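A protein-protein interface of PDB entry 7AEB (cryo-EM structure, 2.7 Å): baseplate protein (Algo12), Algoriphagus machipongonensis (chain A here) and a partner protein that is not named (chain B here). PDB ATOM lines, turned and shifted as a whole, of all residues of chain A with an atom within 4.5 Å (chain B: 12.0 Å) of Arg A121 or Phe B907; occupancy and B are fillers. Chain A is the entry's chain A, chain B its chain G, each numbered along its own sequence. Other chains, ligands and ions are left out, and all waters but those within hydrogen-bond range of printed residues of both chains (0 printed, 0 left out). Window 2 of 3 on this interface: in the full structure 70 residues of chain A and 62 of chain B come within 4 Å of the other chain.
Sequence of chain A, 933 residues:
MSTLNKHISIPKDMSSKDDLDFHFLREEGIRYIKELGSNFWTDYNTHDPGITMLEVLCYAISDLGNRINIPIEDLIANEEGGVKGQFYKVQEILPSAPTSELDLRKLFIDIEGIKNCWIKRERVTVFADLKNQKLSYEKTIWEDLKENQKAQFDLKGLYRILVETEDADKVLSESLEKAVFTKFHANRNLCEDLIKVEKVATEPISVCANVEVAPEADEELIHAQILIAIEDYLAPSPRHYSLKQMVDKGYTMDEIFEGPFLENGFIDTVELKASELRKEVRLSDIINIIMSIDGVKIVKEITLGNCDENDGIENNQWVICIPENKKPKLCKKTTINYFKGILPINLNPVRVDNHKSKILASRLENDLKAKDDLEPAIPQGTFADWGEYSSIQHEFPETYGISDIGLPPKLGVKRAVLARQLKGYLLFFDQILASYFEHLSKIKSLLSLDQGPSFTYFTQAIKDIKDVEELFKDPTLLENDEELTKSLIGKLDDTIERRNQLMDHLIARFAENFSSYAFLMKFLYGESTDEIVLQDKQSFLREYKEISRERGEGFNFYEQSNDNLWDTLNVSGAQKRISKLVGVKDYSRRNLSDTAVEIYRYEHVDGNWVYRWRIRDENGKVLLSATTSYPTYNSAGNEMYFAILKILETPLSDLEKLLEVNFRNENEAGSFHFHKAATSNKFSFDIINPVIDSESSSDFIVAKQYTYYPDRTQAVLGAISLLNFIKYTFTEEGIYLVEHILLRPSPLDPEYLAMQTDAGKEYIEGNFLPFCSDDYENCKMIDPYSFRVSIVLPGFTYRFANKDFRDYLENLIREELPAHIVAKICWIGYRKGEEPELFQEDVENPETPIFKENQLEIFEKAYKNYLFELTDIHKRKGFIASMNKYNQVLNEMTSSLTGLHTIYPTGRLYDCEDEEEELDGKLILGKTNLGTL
The side-chain hydroxyl (OH) of Tyr A159 lies within hydrogen-bond range of a ring nitrogen (NE2) of His B908 (2.8 Å). A ring nitrogen (ND1) of His B908 lies within hydrogen-bond range of the backbone carbonyl oxygen (O) of Lys A156 (3.4 Å).
N of His B908 lies close to OG of Ser B906, at 3.4 Å. O of Leu A155 lies within hydrogen-bond range of NH1 of Arg A121 (3.3 Å).
CA of Ser B906 touches O of Thr A99 (3.8 Å). Glu A101 touches Phe B907 (OE1 to CD1, 3.5 Å). Phe B907 touches Ile A119. Arg A121 touches Phe B907 (CB to CE2, 3.8 Å). Tyr A159 touches Phe B907 (CE2 to CD2, 3.6 Å).
Of the printed residues of chain B, Thr A99 touches Ser B906. Of chain B, only Phe B907 comes within 4 Å of Glu A101. Ile A119 touches just one residue of chain B: Phe B907 (3.9 Å). No residue of chain B comes within 4 Å of Lys A120. Of chain B, only Phe B907 (3.8 Å) comes within 4 Å of Arg A121. No residue of chain B comes within 4 Å of Glu A122. No residue of chain B comes within 4 Å of Arg A123. Of chain B, only His B908 (3.4 Å) comes within 4 Å of Lys A156. Tyr A159 touches two residues of chain B. Glu B903 touches none of the printed residues of chain A. Asn B905 touches none of the printed residues of chain A. Of the printed residues of chain A, Ser B906 touches Thr A99. Of chain A, only Glu A101, Ile A119, Arg A121 and Tyr A159 come within 4 Å of Phe B907. Of the printed residues of chain A, His B908 touches Lys A156 (3.4 Å) and Tyr A159 (2.8 Å).
Of the 11 printed residues of chain A, 6 touch a printed residue of chain B. Hydrophobic or aromatic side chains of chain A that line the printed part of chain B: Tyr A159. Hydrophobic or aromatic side chains of chain B within 4 Å of the printed part of chain A: Phe B907 and His B908. Among the printed residues, 7 pairs touch across the chains. Among the printed residues, no Asp or Glu carboxylate lies within 4 Å of a Lys or Arg side-chain nitrogen of the other chain.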
ATOM      1  N   THR A  99       6.533   2.881 -19.877  1.00  0.00           N
ATOM      2  CA  THR A  99       7.647   3.839 -19.805  1.00  0.00           C
ATOM      3  C   THR A  99       8.810   3.430 -18.881  1.00  0.00           C
ATOM      4  O   THR A  99       9.886   4.049 -18.900  1.00  0.00           O
ATOM      5  CB  THR A  99       7.133   5.230 -19.373  1.00  0.00           C
ATOM      6  OG1 THR A  99       6.123   5.674 -20.286  1.00  0.00           O
ATOM      7  CG2 THR A  99       8.240   6.269 -19.329  1.00  0.00           C
ATOM      8  N   GLU A 101      11.457   0.278 -17.004  1.00  0.00           N
ATOM      9  CA  GLU A 101      12.270  -0.882 -17.401  1.00  0.00           C
ATOM     10  C   GLU A 101      11.435  -2.171 -17.289  1.00  0.00           C
ATOM     11  O   GLU A 101      11.503  -3.018 -18.193  1.00  0.00           O
ATOM     12  CB  GLU A 101      13.502  -1.050 -16.505  1.00  0.00           C
ATOM     13  CG  GLU A 101      13.196  -1.079 -15.021  1.00  0.00           C
ATOM     14  CD  GLU A 101      14.399  -1.262 -14.132  1.00  0.00           C
ATOM     15  OE1 GLU A 101      15.528  -1.084 -14.629  1.00  0.00           O
ATOM     16  OE2 GLU A 101      14.210  -1.406 -12.902  1.00  0.00           O
ATOM     17  N   ILE A 119      17.074  -5.284 -20.361  1.00  0.00           N
ATOM     18  CA  ILE A 119      17.284  -3.997 -21.005  1.00  0.00           C
ATOM     19  C   ILE A 119      18.526  -3.335 -20.447  1.00  0.00           C
ATOM     20  O   ILE A 119      18.607  -3.076 -19.243  1.00  0.00           O
ATOM     21  CB  ILE A 119      16.070  -3.077 -20.790  1.00  0.00           C
ATOM     22  CG1 ILE A 119      14.727  -3.770 -21.225  1.00  0.00           C
ATOM     23  CG2 ILE A 119      16.278  -1.756 -21.508  1.00  0.00           C
ATOM     24  CD1 ILE A 119      14.601  -4.184 -22.685  1.00  0.00           C
ATOM     25  N   LYS A 120      19.474  -3.030 -21.317  1.00  0.00           N
ATOM     26  CA  LYS A 120      20.716  -2.404 -20.913  1.00  0.00           C
ATOM     27  C   LYS A 120      20.873  -1.100 -21.672  1.00  0.00           C
ATOM     28  O   LYS A 120      20.256  -0.911 -22.722  1.00  0.00           O
ATOM     29  CB  LYS A 120      21.898  -3.334 -21.182  1.00  0.00           C
ATOM     30  CG  LYS A 120      21.804  -4.719 -20.500  1.00  0.00           C
ATOM     31  CD  LYS A 120      21.848  -4.632 -18.970  1.00  0.00           C
ATOM     32  CE  LYS A 120      21.876  -6.016 -18.317  1.00  0.00           C
ATOM     33  NZ  LYS A 120      21.789  -5.942 -16.812  1.00  0.00           N
ATOM     34  N   ARG A 121      21.762  -0.247 -21.158  1.00  0.00           N
ATOM     35  CA  ARG A 121      22.008   1.111 -21.672  1.00  0.00           C
ATOM     36  C   ARG A 121      23.328   1.200 -22.426  1.00  0.00           C
ATOM     37  O   ARG A 121      24.350   0.740 -21.896  1.00  0.00           O
ATOM     38  CB  ARG A 121      22.124   2.075 -20.498  1.00  0.00           C
ATOM     39  CG  ARG A 121      22.884   3.351 -20.827  1.00  0.00           C
ATOM     40  CD  ARG A 121      23.372   4.076 -19.602  1.00  0.00           C
ATOM     41  NE  ARG A 121      23.857   5.392 -19.973  1.00  0.00           N
ATOM     42  CZ  ARG A 121      24.464   6.228 -19.144  1.00  0.00           C
ATOM     43  NH1 ARG A 121      24.874   7.406 -19.579  1.00  0.00           N
ATOM     44  NH2 ARG A 121      24.664   5.877 -17.891  1.00  0.00           N
ATOM     45  N   GLU A 122      23.317   1.816 -23.614  1.00  0.00           N
ATOM     46  CA  GLU A 122      24.544   2.041 -24.360  1.00  0.00           C
ATOM     47  C   GLU A 122      25.292   3.255 -23.874  1.00  0.00           C
ATOM     48  O   GLU A 122      24.695   4.262 -23.496  1.00  0.00           O
ATOM     49  CB  GLU A 122      24.249   2.260 -25.839  1.00  0.00           C
ATOM     50  CG  GLU A 122      23.655   1.108 -26.493  1.00  0.00           C
ATOM     51  CD  GLU A 122      24.638   0.044 -26.606  1.00  0.00           C
ATOM     52  OE1 GLU A 122      25.562   0.150 -27.391  1.00  0.00           O
ATOM     53  OE2 GLU A 122      24.531  -0.888 -25.852  1.00  0.00           O
ATOM     54  N   ARG A 123      26.619   3.169 -23.932  1.00  0.00           N
ATOM     55  CA  ARG A 123      27.485   4.304 -23.581  1.00  0.00           C
ATOM     56  C   ARG A 123      28.314   4.656 -24.813  1.00  0.00           C
ATOM     57  O   ARG A 123      29.387   4.069 -25.012  1.00  0.00           O
ATOM     58  CB  ARG A 123      28.374   3.974 -22.377  1.00  0.00           C
ATOM     59  CG  ARG A 123      27.604   3.665 -21.101  1.00  0.00           C
ATOM     60  CD  ARG A 123      28.524   3.385 -19.927  1.00  0.00           C
ATOM     61  NE  ARG A 123      27.787   3.123 -18.696  1.00  0.00           N
ATOM     62  CZ  ARG A 123      27.410   1.917 -18.291  1.00  0.00           C
ATOM     63  NH1 ARG A 123      27.700   0.852 -19.016  1.00  0.00           N
ATOM     64  NH2 ARG A 123      26.745   1.777 -17.156  1.00  0.00           N
ATOM     65  N   LEU A 155      26.786   9.487 -24.051  1.00  0.00           N
ATOM     66  CA  LEU A 155      25.392   9.752 -24.397  1.00  0.00           C
ATOM     67  C   LEU A 155      24.415   9.180 -23.356  1.00  0.00           C
ATOM     68  O   LEU A 155      24.647   8.130 -22.749  1.00  0.00           O
ATOM     69  CB  LEU A 155      25.088   9.249 -25.814  1.00  0.00           C
ATOM     70  CG  LEU A 155      25.450  10.244 -26.985  1.00  0.00           C
ATOM     71  CD1 LEU A 155      26.970  10.489 -27.086  1.00  0.00           C
ATOM     72  CD2 LEU A 155      24.939   9.688 -28.297  1.00  0.00           C
ATOM     73  N   LYS A 156      23.277   9.877 -23.164  1.00  0.00           N
ATOM     74  CA  LYS A 156      22.337   9.575 -22.056  1.00  0.00           C
ATOM     75  C   LYS A 156      21.036   8.797 -22.359  1.00  0.00           C
ATOM     76  O   LYS A 156      20.427   8.346 -21.380  1.00  0.00           O
ATOM     77  CB  LYS A 156      21.947  10.865 -21.323  1.00  0.00           C
ATOM     78  CG  LYS A 156      23.081  11.528 -20.559  1.00  0.00           C
ATOM     79  CD  LYS A 156      22.603  12.273 -19.335  1.00  0.00           C
ATOM     80  CE  LYS A 156      23.743  12.703 -18.439  1.00  0.00           C
ATOM     81  NZ  LYS A 156      23.250  13.130 -17.109  1.00  0.00           N
ATOM     82  N   LEU A 158      20.293   5.898 -24.870  1.00  0.00           N
ATOM     83  CA  LEU A 158      20.282   4.833 -25.866  1.00  0.00           C
ATOM     84  C   LEU A 158      20.203   3.415 -25.284  1.00  0.00           C
ATOM     85  O   LEU A 158      20.843   3.119 -24.273  1.00  0.00           O
ATOM     86  CB  LEU A 158      21.517   5.012 -26.725  1.00  0.00           C
ATOM     87  CG  LEU A 158      21.656   6.391 -27.412  1.00  0.00           C
ATOM     88  CD1 LEU A 158      22.963   6.410 -28.158  1.00  0.00           C
ATOM     89  CD2 LEU A 158      20.468   6.666 -28.344  1.00  0.00           C
ATOM     90  N   TYR A 159      19.469   2.519 -25.972  1.00  0.00           N
ATOM     91  CA  TYR A 159      19.253   1.130 -25.532  1.00  0.00           C
ATOM     92  C   TYR A 159      19.853  -0.020 -26.366  1.00  0.00           C
ATOM     93  O   TYR A 159      19.981   0.042 -27.600  1.00  0.00           O
ATOM     94  CB  TYR A 159      17.759   0.811 -25.465  1.00  0.00           C
ATOM     95  CG  TYR A 159      16.975   1.559 -24.476  1.00  0.00           C
ATOM     96  CD1 TYR A 159      16.208   2.629 -24.861  1.00  0.00           C
ATOM     97  CD2 TYR A 159      17.001   1.184 -23.168  1.00  0.00           C
ATOM     98  CE1 TYR A 159      15.474   3.309 -23.937  1.00  0.00           C
ATOM     99  CE2 TYR A 159      16.272   1.849 -22.235  1.00  0.00           C
ATOM    100  CZ  TYR A 159      15.507   2.917 -22.616  1.00  0.00           C
ATOM    101  OH  TYR A 159      14.770   3.602 -21.670  1.00  0.00           O
ATOM    102  N   LYS B 829      -0.342   5.912 -12.236  1.00  0.00           N
ATOM    103  CA  LYS B 829       0.717   5.435 -11.350  1.00  0.00           C
ATOM    104  C   LYS B 829       2.107   5.583 -11.993  1.00  0.00           C
ATOM    105  O   LYS B 829       3.017   4.804 -11.738  1.00  0.00           O
ATOM    106  CB  LYS B 829       0.423   3.988 -10.915  1.00  0.00           C
ATOM    107  CG  LYS B 829       1.193   3.378  -9.766  1.00  0.00           C
ATOM    108  CD  LYS B 829       0.770   3.907  -8.453  1.00  0.00           C
ATOM    109  CE  LYS B 829       1.463   3.141  -7.356  1.00  0.00           C
ATOM    110  NZ  LYS B 829       0.934   3.488  -6.017  1.00  0.00           N
ATOM    111  N   ARG B 830       2.315   6.588 -12.837  1.00  0.00           N
ATOM    112  CA  ARG B 830       3.624   6.846 -13.428  1.00  0.00           C
ATOM    113  C   ARG B 830       4.133   8.185 -12.924  1.00  0.00           C
ATOM    114  O   ARG B 830       3.351   9.109 -12.735  1.00  0.00           O
ATOM    115  CB  ARG B 830       3.567   6.890 -14.951  1.00  0.00           C
ATOM    116  CG  ARG B 830       2.978   5.678 -15.649  1.00  0.00           C
ATOM    117  CD  ARG B 830       3.917   4.521 -15.676  1.00  0.00           C
ATOM    118  NE  ARG B 830       3.646   3.597 -14.586  1.00  0.00           N
ATOM    119  CZ  ARG B 830       4.419   2.566 -14.262  1.00  0.00           C
ATOM    120  NH1 ARG B 830       5.527   2.322 -14.939  1.00  0.00           N
ATOM    121  NH2 ARG B 830       4.080   1.781 -13.254  1.00  0.00           N
ATOM    122  N   ALA B 831       5.436   8.314 -12.708  1.00  0.00           N
ATOM    123  CA  ALA B 831       5.993   9.589 -12.256  1.00  0.00           C
ATOM    124  C   ALA B 831       6.620  10.347 -13.422  1.00  0.00           C
ATOM    125  O   ALA B 831       7.826  10.309 -13.610  1.00  0.00           O
ATOM    126  CB  ALA B 831       7.033   9.339 -11.175  1.00  0.00           C
ATOM    127  N   ILE B 832       5.830  11.057 -14.223  1.00  0.00           N
ATOM    128  CA  ILE B 832       6.386  11.712 -15.407  1.00  0.00           C
ATOM    129  C   ILE B 832       6.526  13.226 -15.239  1.00  0.00           C
ATOM    130  O   ILE B 832       7.615  13.767 -15.411  1.00  0.00           O
ATOM    131  CB  ILE B 832       5.582  11.350 -16.671  1.00  0.00           C
ATOM    132  CG1 ILE B 832       5.702   9.841 -16.881  1.00  0.00           C
ATOM    133  CG2 ILE B 832       6.081  12.147 -17.880  1.00  0.00           C
ATOM    134  CD1 ILE B 832       4.775   9.277 -17.905  1.00  0.00           C
ATOM    135  N   TYR B 837       4.601  13.654  -9.680  1.00  0.00           N
ATOM    136  CA  TYR B 837       5.530  13.422  -8.578  1.00  0.00           C
ATOM    137  C   TYR B 837       4.976  13.926  -7.257  1.00  0.00           C
ATOM    138  O   TYR B 837       5.050  13.234  -6.234  1.00  0.00           O
ATOM    139  CB  TYR B 837       6.853  14.133  -8.827  1.00  0.00           C
ATOM    140  CG  TYR B 837       7.829  13.481  -9.760  1.00  0.00           C
ATOM    141  CD1 TYR B 837       8.664  12.491  -9.324  1.00  0.00           C
ATOM    142  CD2 TYR B 837       7.958  13.908 -11.052  1.00  0.00           C
ATOM    143  CE1 TYR B 837       9.571  11.925 -10.168  1.00  0.00           C
ATOM    144  CE2 TYR B 837       8.835  13.357 -11.914  1.00  0.00           C
ATOM    145  CZ  TYR B 837       9.647  12.361 -11.469  1.00  0.00           C
ATOM    146  OH  TYR B 837      10.550  11.803 -12.333  1.00  0.00           O
ATOM    147  N   PRO B 865      19.962  18.630 -17.564  1.00  0.00           N
ATOM    148  CA  PRO B 865      18.954  17.700 -18.069  1.00  0.00           C
ATOM    149  C   PRO B 865      19.207  16.309 -17.532  1.00  0.00           C
ATOM    150  O   PRO B 865      20.336  15.959 -17.199  1.00  0.00           O
ATOM    151  CB  PRO B 865      19.170  17.756 -19.586  1.00  0.00           C
ATOM    152  CG  PRO B 865      20.610  18.126 -19.735  1.00  0.00           C
ATOM    153  CD  PRO B 865      20.942  19.017 -18.583  1.00  0.00           C
ATOM    154  N   GLY B 866      18.144  15.514 -17.450  1.00  0.00           N
ATOM    155  CA  GLY B 866      18.285  14.132 -17.043  1.00  0.00           C
ATOM    156  C   GLY B 866      18.347  13.906 -15.552  1.00  0.00           C
ATOM    157  O   GLY B 866      18.899  12.899 -15.107  1.00  0.00           O
ATOM    158  N   ASN B 867      17.775  14.799 -14.758  1.00  0.00           N
ATOM    159  CA  ASN B 867      17.842  14.659 -13.314  1.00  0.00           C
ATOM    160  C   ASN B 867      16.649  15.378 -12.699  1.00  0.00           C
ATOM    161  O   ASN B 867      15.869  16.012 -13.410  1.00  0.00           O
ATOM    162  CB  ASN B 867      19.164  15.227 -12.823  1.00  0.00           C
ATOM    163  CG  ASN B 867      19.672  14.541 -11.611  1.00  0.00           C
ATOM    164  OD1 ASN B 867      18.914  14.170 -10.715  1.00  0.00           O
ATOM    165  ND2 ASN B 867      20.975  14.373 -11.556  1.00  0.00           N
ATOM    166  N   ALA B 898      12.876   8.322  -2.206  1.00  0.00           N
ATOM    167  CA  ALA B 898      13.689   8.168  -3.401  1.00  0.00           C
ATOM    168  C   ALA B 898      13.481   6.814  -4.050  1.00  0.00           C
ATOM    169  O   ALA B 898      13.304   6.737  -5.269  1.00  0.00           O
ATOM    170  CB  ALA B 898      15.157   8.351  -3.060  1.00  0.00           C
ATOM    171  N   ALA B 899      13.433   5.751  -3.248  1.00  0.00           N
ATOM    172  CA  ALA B 899      13.258   4.411  -3.797  1.00  0.00           C
ATOM    173  C   ALA B 899      11.920   4.267  -4.501  1.00  0.00           C
ATOM    174  O   ALA B 899      11.858   3.770  -5.632  1.00  0.00           O
ATOM    175  CB  ALA B 899      13.361   3.380  -2.685  1.00  0.00           C
ATOM    176  N   PHE B 900      10.859   4.754  -3.854  1.00  0.00           N
ATOM    177  CA  PHE B 900       9.491   4.659  -4.358  1.00  0.00           C
ATOM    178  C   PHE B 900       9.353   5.297  -5.726  1.00  0.00           C
ATOM    179  O   PHE B 900       8.782   4.711  -6.644  1.00  0.00           O
ATOM    180  CB  PHE B 900       8.556   5.335  -3.359  1.00  0.00           C
ATOM    181  CG  PHE B 900       7.169   5.568  -3.859  1.00  0.00           C
ATOM    182  CD1 PHE B 900       6.259   4.543  -3.958  1.00  0.00           C
ATOM    183  CD2 PHE B 900       6.767   6.842  -4.185  1.00  0.00           C
ATOM    184  CE1 PHE B 900       4.981   4.799  -4.404  1.00  0.00           C
ATOM    185  CE2 PHE B 900       5.505   7.099  -4.624  1.00  0.00           C
ATOM    186  CZ  PHE B 900       4.610   6.086  -4.736  1.00  0.00           C
ATOM    187  N   VAL B 901       9.804   6.520  -5.821  1.00  0.00           N
ATOM    188  CA  VAL B 901       9.781   7.249  -7.051  1.00  0.00           C
ATOM    189  C   VAL B 901      10.697   6.751  -8.158  1.00  0.00           C
ATOM    190  O   VAL B 901      10.329   6.796  -9.307  1.00  0.00           O
ATOM    191  CB  VAL B 901      10.018   8.729  -6.787  1.00  0.00           C
ATOM    192  CG1 VAL B 901      10.243   9.458  -8.092  1.00  0.00           C
ATOM    193  CG2 VAL B 901       8.814   9.296  -6.072  1.00  0.00           C
ATOM    194  N   ASN B 902      11.903   6.302  -7.830  1.00  0.00           N
ATOM    195  CA  ASN B 902      12.832   5.914  -8.880  1.00  0.00           C
ATOM    196  C   ASN B 902      12.331   4.687  -9.641  1.00  0.00           C
ATOM    197  O   ASN B 902      12.413   4.660 -10.874  1.00  0.00           O
ATOM    198  CB  ASN B 902      14.224   5.769  -8.280  1.00  0.00           C
ATOM    199  CG  ASN B 902      14.830   7.148  -7.993  1.00  0.00           C
ATOM    200  OD1 ASN B 902      14.383   8.129  -8.578  1.00  0.00           O
ATOM    201  ND2 ASN B 902      15.796   7.239  -7.097  1.00  0.00           N
ATOM    202  N   GLU B 903      11.624   3.780  -8.956  1.00  0.00           N
ATOM    203  CA  GLU B 903      10.932   2.666  -9.613  1.00  0.00           C
ATOM    204  C   GLU B 903       9.869   3.042 -10.627  1.00  0.00           C
ATOM    205  O   GLU B 903       9.548   2.215 -11.489  1.00  0.00           O
ATOM    206  CB  GLU B 903      10.315   1.695  -8.600  1.00  0.00           C
ATOM    207  CG  GLU B 903      11.245   1.151  -7.554  1.00  0.00           C
ATOM    208  CD  GLU B 903      10.548   0.289  -6.528  1.00  0.00           C
ATOM    209  OE1 GLU B 903       9.327   0.410  -6.392  1.00  0.00           O
ATOM    210  OE2 GLU B 903      11.225  -0.451  -5.804  1.00  0.00           O
ATOM    211  N   LEU B 904       9.298   4.232 -10.528  1.00  0.00           N
ATOM    212  CA  LEU B 904       8.213   4.674 -11.389  1.00  0.00           C
ATOM    213  C   LEU B 904       8.623   5.719 -12.409  1.00  0.00           C
ATOM    214  O   LEU B 904       7.751   6.273 -13.078  1.00  0.00           O
ATOM    215  CB  LEU B 904       7.088   5.279 -10.549  1.00  0.00           C
ATOM    216  CG  LEU B 904       6.411   4.442  -9.479  1.00  0.00           C
ATOM    217  CD1 LEU B 904       5.415   5.320  -8.724  1.00  0.00           C
ATOM    218  CD2 LEU B 904       5.733   3.256 -10.117  1.00  0.00           C
ATOM    219  N   ASN B 905       9.890   6.090 -12.492  1.00  0.00           N
ATOM    220  CA  ASN B 905      10.220   7.234 -13.348  1.00  0.00           C
ATOM    221  C   ASN B 905      10.445   6.854 -14.799  1.00  0.00           C
ATOM    222  O   ASN B 905       9.647   7.169 -15.688  1.00  0.00           O
ATOM    223  CB  ASN B 905      11.525   7.878 -12.915  1.00  0.00           C
ATOM    224  CG  ASN B 905      11.450   8.624 -11.661  1.00  0.00           C
ATOM    225  OD1 ASN B 905      10.396   9.008 -11.164  1.00  0.00           O
ATOM    226  ND2 ASN B 905      12.619   8.877 -11.124  1.00  0.00           N
ATOM    227  N   SER B 906      11.562   6.198 -15.023  1.00  0.00           N
ATOM    228  CA  SER B 906      12.076   5.824 -16.317  1.00  0.00           C
ATOM    229  C   SER B 906      13.343   5.070 -16.055  1.00  0.00           C
ATOM    230  O   SER B 906      14.039   5.363 -15.078  1.00  0.00           O
ATOM    231  CB  SER B 906      12.397   7.018 -17.199  1.00  0.00           C
ATOM    232  OG  SER B 906      13.057   6.580 -18.364  1.00  0.00           O
ATOM    233  N   PHE B 907      13.670   4.161 -16.961  1.00  0.00           N
ATOM    234  CA  PHE B 907      14.933   3.450 -16.877  1.00  0.00           C
ATOM    235  C   PHE B 907      16.130   4.392 -16.710  1.00  0.00           C
ATOM    236  O   PHE B 907      17.066   4.089 -15.968  1.00  0.00           O
ATOM    237  CB  PHE B 907      15.123   2.602 -18.121  1.00  0.00           C
ATOM    238  CG  PHE B 907      16.417   1.919 -18.129  1.00  0.00           C
ATOM    239  CD1 PHE B 907      16.631   0.837 -17.315  1.00  0.00           C
ATOM    240  CD2 PHE B 907      17.443   2.384 -18.908  1.00  0.00           C
ATOM    241  CE1 PHE B 907      17.845   0.224 -17.299  1.00  0.00           C
ATOM    242  CE2 PHE B 907      18.653   1.783 -18.888  1.00  0.00           C
ATOM    243  CZ  PHE B 907      18.857   0.701 -18.088  1.00  0.00           C
ATOM    244  N   HIS B 908      16.081   5.557 -17.344  1.00  0.00           N
ATOM    245  CA  HIS B 908      17.207   6.469 -17.383  1.00  0.00           C
ATOM    246  C   HIS B 908      17.250   7.537 -16.290  1.00  0.00           C
ATOM    247  O   HIS B 908      18.146   8.384 -16.346  1.00  0.00           O
ATOM    248  CB  HIS B 908      17.212   7.190 -18.720  1.00  0.00           C
ATOM    249  CG  HIS B 908      17.383   6.290 -19.889  1.00  0.00           C
ATOM    250  ND1 HIS B 908      18.594   5.733 -20.227  1.00  0.00           N
ATOM    251  CD2 HIS B 908      16.495   5.855 -20.810  1.00  0.00           C
ATOM    252  CE1 HIS B 908      18.446   4.991 -21.308  1.00  0.00           C
ATOM    253  NE2 HIS B 908      17.181   5.048 -21.681  1.00  0.00           N
ATOM    254  N   VAL B 909      16.309   7.618 -15.342  1.00  0.00           N
ATOM    255  CA  VAL B 909      16.316   8.771 -14.428  1.00  0.00           C
ATOM    256  C   VAL B 909      16.209   8.410 -12.945  1.00  0.00           C
ATOM    257  O   VAL B 909      15.275   7.722 -12.511  1.00  0.00           O
ATOM    258  CB  VAL B 909      15.221   9.794 -14.783  1.00  0.00           C
ATOM    259  CG1 VAL B 909      15.206  10.966 -13.768  1.00  0.00           C
ATOM    260  CG2 VAL B 909      15.459  10.354 -16.169  1.00  0.00           C
ATOM    261  N   GLN B 910      17.133   8.953 -12.157  1.00  0.00           N
ATOM    262  CA  GLN B 910      17.083   8.871 -10.712  1.00  0.00           C
ATOM    263  C   GLN B 910      16.830  10.245 -10.124  1.00  0.00           C
ATOM    264  O   GLN B 910      17.428  11.227 -10.563  1.00  0.00           O
ATOM    265  CB  GLN B 910      18.381   8.303 -10.129  1.00  0.00           C
ATOM    266  CG  GLN B 910      18.701   6.958 -10.692  1.00  0.00           C
ATOM    267  CD  GLN B 910      17.933   5.868  -9.974  1.00  0.00           C
ATOM    268  OE1 GLN B 910      17.888   5.800  -8.748  1.00  0.00           O
ATOM    269  NE2 GLN B 910      17.209   5.074 -10.761  1.00  0.00           N
ATOM    270  N   ALA B 911      15.962  10.321  -9.121  1.00  0.00           N
ATOM    271  CA  ALA B 911      15.692  11.577  -8.442  1.00  0.00           C
ATOM    272  C   ALA B 911      16.394  11.614  -7.097  1.00  0.00           C
ATOM    273  O   ALA B 911      16.657  10.577  -6.482  1.00  0.00           O
ATOM    274  CB  ALA B 911      14.192  11.789  -8.242  1.00  0.00           C
